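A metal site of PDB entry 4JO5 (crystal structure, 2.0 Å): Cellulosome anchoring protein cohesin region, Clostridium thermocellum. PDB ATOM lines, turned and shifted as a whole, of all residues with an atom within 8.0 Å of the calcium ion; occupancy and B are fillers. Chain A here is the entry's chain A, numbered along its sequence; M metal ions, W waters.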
ATOM      1  N   ASP A  30      23.541  -0.063 -32.549  1.00  0.00           N
ATOM      2  CA  ASP A  30      24.496  -0.233 -31.458  1.00  0.00           C
ATOM      3  C   ASP A  30      24.205   0.807 -30.395  1.00  0.00           C
ATOM      4  O   ASP A  30      24.147   0.484 -29.201  1.00  0.00           O
ATOM      5  CB  ASP A  30      25.939  -0.131 -31.956  1.00  0.00           C
ATOM      6  CG  ASP A  30      26.949  -0.253 -30.836  1.00  0.00           C
ATOM      7  OD1 ASP A  30      26.810  -1.181 -29.991  1.00  0.00           O
ATOM      8  OD2 ASP A  30      27.877   0.588 -30.793  1.00  0.00           O
ATOM      9  N   ILE A  35      15.971  -0.931 -25.581  1.00  0.00           N
ATOM     10  CA  ILE A  35      16.374  -2.284 -25.924  1.00  0.00           C
ATOM     11  C   ILE A  35      15.078  -3.100 -26.044  1.00  0.00           C
ATOM     12  O   ILE A  35      14.157  -2.921 -25.238  1.00  0.00           O
ATOM     13  CB  ILE A  35      17.343  -2.805 -24.841  1.00  0.00           C
ATOM     14  CG1 ILE A  35      18.642  -1.975 -24.935  1.00  0.00           C
ATOM     15  CG2 ILE A  35      17.603  -4.289 -25.018  1.00  0.00           C
ATOM     16  CD1 ILE A  35      19.586  -2.101 -23.771  1.00  0.00           C
ATOM     17  N   TYR A  59      20.660 -10.379 -19.931  1.00  0.00           N
ATOM     18  CA  TYR A  59      21.863  -9.838 -19.283  1.00  0.00           C
ATOM     19  C   TYR A  59      22.486  -8.758 -20.176  1.00  0.00           C
ATOM     20  O   TYR A  59      22.628  -8.952 -21.374  1.00  0.00           O
ATOM     21  CB  TYR A  59      22.905 -10.950 -19.039  1.00  0.00           C
ATOM     22  CG  TYR A  59      22.556 -11.977 -17.962  1.00  0.00           C
ATOM     23  CD1 TYR A  59      22.906 -11.760 -16.638  1.00  0.00           C
ATOM     24  CD2 TYR A  59      21.884 -13.173 -18.258  1.00  0.00           C
ATOM     25  CE1 TYR A  59      22.610 -12.664 -15.645  1.00  0.00           C
ATOM     26  CE2 TYR A  59      21.582 -14.120 -17.234  1.00  0.00           C
ATOM     27  CZ  TYR A  59      21.957 -13.848 -15.932  1.00  0.00           C
ATOM     28  OH  TYR A  59      21.697 -14.721 -14.873  1.00  0.00           O
ATOM     29  N   TYR A  60      22.874  -7.644 -19.575  1.00  0.00           N
ATOM     30  CA  TYR A  60      23.413  -6.519 -20.355  1.00  0.00           C
ATOM     31  C   TYR A  60      24.247  -5.623 -19.464  1.00  0.00           C
ATOM     32  O   TYR A  60      24.348  -5.856 -18.249  1.00  0.00           O
ATOM     33  CB  TYR A  60      22.282  -5.735 -21.042  1.00  0.00           C
ATOM     34  CG  TYR A  60      21.309  -5.029 -20.112  1.00  0.00           C
ATOM     35  CD1 TYR A  60      20.342  -5.736 -19.401  1.00  0.00           C
ATOM     36  CD2 TYR A  60      21.331  -3.635 -19.959  1.00  0.00           C
ATOM     37  CE1 TYR A  60      19.432  -5.093 -18.565  1.00  0.00           C
ATOM     38  CE2 TYR A  60      20.428  -2.975 -19.113  1.00  0.00           C
ATOM     39  CZ  TYR A  60      19.470  -3.718 -18.430  1.00  0.00           C
ATOM     40  OH  TYR A  60      18.583  -3.077 -17.584  1.00  0.00           O
ATOM     41  N   THR A  61      24.904  -4.635 -20.065  1.00  0.00           N
ATOM     42  CA  THR A  61      25.579  -3.574 -19.317  1.00  0.00           C
ATOM     43  C   THR A  61      24.788  -2.270 -19.423  1.00  0.00           C
ATOM     44  O   THR A  61      24.488  -1.805 -20.515  1.00  0.00           O
ATOM     45  CB  THR A  61      26.986  -3.307 -19.855  1.00  0.00           C
ATOM     46  OG1 THR A  61      26.927  -3.102 -21.262  1.00  0.00           O
ATOM     47  CG2 THR A  61      27.929  -4.459 -19.551  1.00  0.00           C
ATOM     48  N   VAL A  62      24.476  -1.671 -18.285  1.00  0.00           N
ATOM     49  CA  VAL A  62      23.551  -0.533 -18.254  1.00  0.00           C
ATOM     50  C   VAL A  62      24.179   0.739 -18.850  1.00  0.00           C
ATOM     51  O   VAL A  62      23.468   1.644 -19.272  1.00  0.00           O
ATOM     52  CB  VAL A  62      23.088  -0.241 -16.792  1.00  0.00           C
ATOM     53  CG1 VAL A  62      24.270   0.189 -15.923  1.00  0.00           C
ATOM     54  CG2 VAL A  62      21.989   0.848 -16.777  1.00  0.00           C
ATOM     55  N   ASP A  63      25.514   0.814 -18.865  1.00  0.00           N
ATOM     56  CA  ASP A  63      26.221   1.933 -19.522  1.00  0.00           C
ATOM     57  C   ASP A  63      25.863   3.269 -18.892  1.00  0.00           C
ATOM     58  O   ASP A  63      25.312   4.147 -19.554  1.00  0.00           O
ATOM     59  CB  ASP A  63      25.886   2.024 -21.018  1.00  0.00           C
ATOM     60  CG  ASP A  63      25.980   0.690 -21.731  1.00  0.00           C
ATOM     61  OD1 ASP A  63      26.986  -0.020 -21.544  1.00  0.00           O
ATOM     62  OD2 ASP A  63      25.035   0.369 -22.480  1.00  0.00           O
ATOM     63  N   GLY A  64      26.155   3.408 -17.607  1.00  0.00           N
ATOM     64  CA  GLY A  64      25.872   4.647 -16.890  1.00  0.00           C
ATOM     65  C   GLY A  64      24.623   4.349 -16.088  1.00  0.00           C
ATOM     66  O   GLY A  64      23.537   4.332 -16.629  1.00  0.00           O
ATOM     67  N   ASN A 103      32.249  -9.016 -17.925  1.00  0.00           N
ATOM     68  CA  ASN A 103      32.574  -7.909 -18.842  1.00  0.00           C
ATOM     69  C   ASN A 103      31.391  -7.333 -19.602  1.00  0.00           C
ATOM     70  O   ASN A 103      31.287  -6.112 -19.781  1.00  0.00           O
ATOM     71  CB  ASN A 103      33.630  -8.342 -19.853  1.00  0.00           C
ATOM     72  CG  ASN A 103      35.036  -7.990 -19.393  1.00  0.00           C
ATOM     73  OD1 ASN A 103      35.281  -6.880 -18.933  1.00  0.00           O
ATOM     74  ND2 ASN A 103      35.951  -8.952 -19.479  1.00  0.00           N
ATOM     75  N   ASN A 104      30.497  -8.224 -20.027  1.00  0.00           N
ATOM     76  CA  ASN A 104      29.286  -7.819 -20.778  1.00  0.00           C
ATOM     77  C   ASN A 104      27.978  -7.978 -20.019  1.00  0.00           C
ATOM     78  O   ASN A 104      26.922  -8.028 -20.642  1.00  0.00           O
ATOM     79  CB  ASN A 104      29.223  -8.619 -22.062  1.00  0.00           C
ATOM     80  CG  ASN A 104      30.352  -8.284 -22.986  1.00  0.00           C
ATOM     81  OD1 ASN A 104      30.626  -7.107 -23.238  1.00  0.00           O
ATOM     82  ND2 ASN A 104      31.052  -9.302 -23.456  1.00  0.00           N
ATOM     83  N   ALA A 105      28.043  -8.049 -18.688  1.00  0.00           N
ATOM     84  CA  ALA A 105      26.822  -8.089 -17.894  1.00  0.00           C
ATOM     85  C   ALA A 105      27.085  -7.477 -16.532  1.00  0.00           C
ATOM     86  O   ALA A 105      27.950  -7.973 -15.808  1.00  0.00           O
ATOM     87  CB  ALA A 105      26.350  -9.546 -17.733  1.00  0.00           C
ATOM     88  N   ASP A 106      26.380  -6.393 -16.198  1.00  0.00           N
ATOM     89  CA  ASP A 106      26.367  -5.914 -14.819  1.00  0.00           C
ATOM     90  C   ASP A 106      24.929  -5.877 -14.287  1.00  0.00           C
ATOM     91  O   ASP A 106      24.708  -5.583 -13.101  1.00  0.00           O
ATOM     92  CB  ASP A 106      27.029  -4.531 -14.669  1.00  0.00           C
ATOM     93  CG  ASP A 106      26.462  -3.486 -15.634  1.00  0.00           C
ATOM     94  OD1 ASP A 106      25.243  -3.470 -15.902  1.00  0.00           O
ATOM     95  OD2 ASP A 106      27.256  -2.676 -16.137  1.00  0.00           O
ATOM     96  N   LYS A 132      16.193   3.591 -20.052  1.00  0.00           N
ATOM     97  CA  LYS A 132      16.529   4.397 -18.894  1.00  0.00           C
ATOM     98  C   LYS A 132      15.515   5.527 -18.799  1.00  0.00           C
ATOM     99  O   LYS A 132      15.021   5.986 -19.810  1.00  0.00           O
ATOM    100  CB  LYS A 132      17.958   4.913 -19.022  1.00  0.00           C
ATOM    101  CG  LYS A 132      18.951   3.796 -19.030  1.00  0.00           C
ATOM    102  CD  LYS A 132      20.364   4.281 -18.930  1.00  0.00           C
ATOM    103  CE  LYS A 132      21.052   4.212 -20.248  1.00  0.00           C
ATOM    104  NZ  LYS A 132      22.513   4.162 -20.010  1.00  0.00           N
ATOM    105  N   ASN A 137      21.140   7.056 -23.949  1.00  0.00           N
ATOM    106  CA  ASN A 137      21.529   5.921 -24.770  1.00  0.00           C
ATOM    107  C   ASN A 137      22.200   4.752 -24.038  1.00  0.00           C
ATOM    108  O   ASN A 137      22.898   4.911 -23.034  1.00  0.00           O
ATOM    109  CB  ASN A 137      22.414   6.402 -25.912  1.00  0.00           C
ATOM    110  CG  ASN A 137      21.630   7.192 -26.938  1.00  0.00           C
ATOM    111  OD1 ASN A 137      20.480   6.890 -27.236  1.00  0.00           O
ATOM    112  ND2 ASN A 137      22.251   8.219 -27.481  1.00  0.00           N
ATOM    113  N   TYR A 138      21.916   3.581 -24.573  1.00  0.00           N
ATOM    114  CA  TYR A 138      22.610   2.359 -24.251  1.00  0.00           C
ATOM    115  C   TYR A 138      23.563   2.082 -25.402  1.00  0.00           C
ATOM    116  O   TYR A 138      23.403   2.625 -26.483  1.00  0.00           O
ATOM    117  CB  TYR A 138      21.640   1.188 -24.224  1.00  0.00           C
ATOM    118  CG  TYR A 138      20.639   1.116 -23.106  1.00  0.00           C
ATOM    119  CD1 TYR A 138      21.015   0.738 -21.825  1.00  0.00           C
ATOM    120  CD2 TYR A 138      19.277   1.300 -23.356  1.00  0.00           C
ATOM    121  CE1 TYR A 138      20.073   0.587 -20.812  1.00  0.00           C
ATOM    122  CE2 TYR A 138      18.329   1.177 -22.343  1.00  0.00           C
ATOM    123  CZ  TYR A 138      18.715   0.807 -21.081  1.00  0.00           C
ATOM    124  OH  TYR A 138      17.769   0.692 -20.080  1.00  0.00           O
ATOM    125  N   THR A 139      24.520   1.198 -25.152  1.00  0.00           N
ATOM    126  CA  THR A 139      25.328   0.592 -26.197  1.00  0.00           C
ATOM    127  C   THR A 139      25.031  -0.886 -26.162  1.00  0.00           C
ATOM    128  O   THR A 139      25.233  -1.501 -25.109  1.00  0.00           O
ATOM    129  CB  THR A 139      26.800   0.785 -25.896  1.00  0.00           C
ATOM    130  OG1 THR A 139      27.091   2.182 -25.956  1.00  0.00           O
ATOM    131  CG2 THR A 139      27.676   0.022 -26.892  1.00  0.00           C
ATOM    132  N   GLN A 140      24.582  -1.461 -27.283  1.00  0.00           N
ATOM    133  CA  GLN A 140      24.174  -2.862 -27.302  1.00  0.00           C
ATOM    134  C   GLN A 140      25.311  -3.873 -27.573  1.00  0.00           C
ATOM    135  O   GLN A 140      25.197  -5.037 -27.204  1.00  0.00           O
ATOM    136  CB  GLN A 140      23.062  -3.089 -28.330  1.00  0.00           C
ATOM    137  CG  GLN A 140      21.808  -2.246 -28.062  1.00  0.00           C
ATOM    138  CD  GLN A 140      20.587  -2.883 -28.688  1.00  0.00           C
ATOM    139  OE1 GLN A 140      19.931  -3.698 -28.065  1.00  0.00           O
ATOM    140  NE2 GLN A 140      20.321  -2.540 -29.938  1.00  0.00           N
ATOM    141  N   SER A 141      26.423  -3.415 -28.160  1.00  0.00           N
ATOM    142  CA  SER A 141      27.563  -4.282 -28.460  1.00  0.00           C
ATOM    143  C   SER A 141      28.333  -4.858 -27.235  1.00  0.00           C
ATOM    144  O   SER A 141      29.126  -5.796 -27.383  1.00  0.00           O
ATOM    145  CB  SER A 141      28.538  -3.567 -29.398  1.00  0.00           C
ATOM    146  OG  SER A 141      29.123  -2.448 -28.763  1.00  0.00           O
ATOM    147  N   ASN A 142      28.125  -4.310 -26.044  1.00  0.00           N
ATOM    148  CA  ASN A 142      28.701  -4.903 -24.834  1.00  0.00           C
ATOM    149  C   ASN A 142      27.624  -5.517 -23.935  1.00  0.00           C
ATOM    150  O   ASN A 142      27.715  -5.434 -22.700  1.00  0.00           O
ATOM    151  CB  ASN A 142      29.506  -3.859 -24.058  1.00  0.00           C
ATOM    152  CG  ASN A 142      28.677  -2.639 -23.689  1.00  0.00           C
ATOM    153  OD1 ASN A 142      27.472  -2.589 -23.902  1.00  0.00           O
ATOM    154  ND2 ASN A 142      29.339  -1.637 -23.110  1.00  0.00           N
ATOM    155  N   ASP A 143      26.613  -6.113 -24.552  1.00  0.00           N
ATOM    156  CA  ASP A 143      25.517  -6.759 -23.842  1.00  0.00           C
ATOM    157  C   ASP A 143      25.474  -8.263 -24.121  1.00  0.00           C
ATOM    158  O   ASP A 143      25.216  -8.715 -25.254  1.00  0.00           O
ATOM    159  CB  ASP A 143      24.167  -6.152 -24.228  1.00  0.00           C
ATOM    160  CG  ASP A 143      23.983  -4.702 -23.776  1.00  0.00           C
ATOM    161  OD1 ASP A 143      24.801  -4.166 -22.977  1.00  0.00           O
ATOM    162  OD2 ASP A 143      23.000  -4.083 -24.238  1.00  0.00           O
ATOM    163  N   TYR A 144      25.693  -9.027 -23.062  1.00  0.00           N
ATOM    164  CA  TYR A 144      25.832 -10.481 -23.159  1.00  0.00           C
ATOM    165  C   TYR A 144      24.671 -11.099 -23.962  1.00  0.00           C
ATOM    166  O   TYR A 144      24.921 -11.861 -24.891  1.00  0.00           O
ATOM    167  CB  TYR A 144      25.906 -11.059 -21.746  1.00  0.00           C
ATOM    168  CG  TYR A 144      26.032 -12.574 -21.665  1.00  0.00           C
ATOM    169  CD1 TYR A 144      27.264 -13.205 -21.901  1.00  0.00           C
ATOM    170  CD2 TYR A 144      24.938 -13.363 -21.330  1.00  0.00           C
ATOM    171  CE1 TYR A 144      27.376 -14.586 -21.826  1.00  0.00           C
ATOM    172  CE2 TYR A 144      25.043 -14.745 -21.231  1.00  0.00           C
ATOM    173  CZ  TYR A 144      26.261 -15.350 -21.479  1.00  0.00           C
ATOM    174  OH  TYR A 144      26.353 -16.706 -21.392  1.00  0.00           O
HETATM  175 CA    CA M   1      25.427  -1.942 -22.731  1.00  0.00          CA
HETATM  176  O   HOH W   1      22.978  -1.762 -23.141  1.00  0.00           O
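The backbone carbonyl oxygen of Asn 142 sits close to the side-chain amide oxygen of Asn 104.
O of Asp 63 lies within hydrogen-bond range of NZ of Lys 132 (2.8 Å).
Five residues have an atom within 4 Å of the calcium ion: Thr 61, Asp 63, Thr 139, Asn 142 and Asp 143.
The side-chain carboxylate (OD1) of Asp 143 is bound to the calcium ion (2.3 Å).
The calcium ion is bound by OD2 of Asp 63 (2.4 Å).
OG1 of Thr 61 is bound to the calcium ion (2.4 Å).
O of Thr 61 binds the calcium ion.
O of Thr 139 is bound to the calcium ion, 2.4 Å away.
The calcium ion is bound by OD1 of Asn 142, 2.4 Å away.
Water W1 binds the calcium ion (2.5 Å).
The side-chain carboxylate (OD1) of Asp 63 binds the calcium ion, at 2.7 Å.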
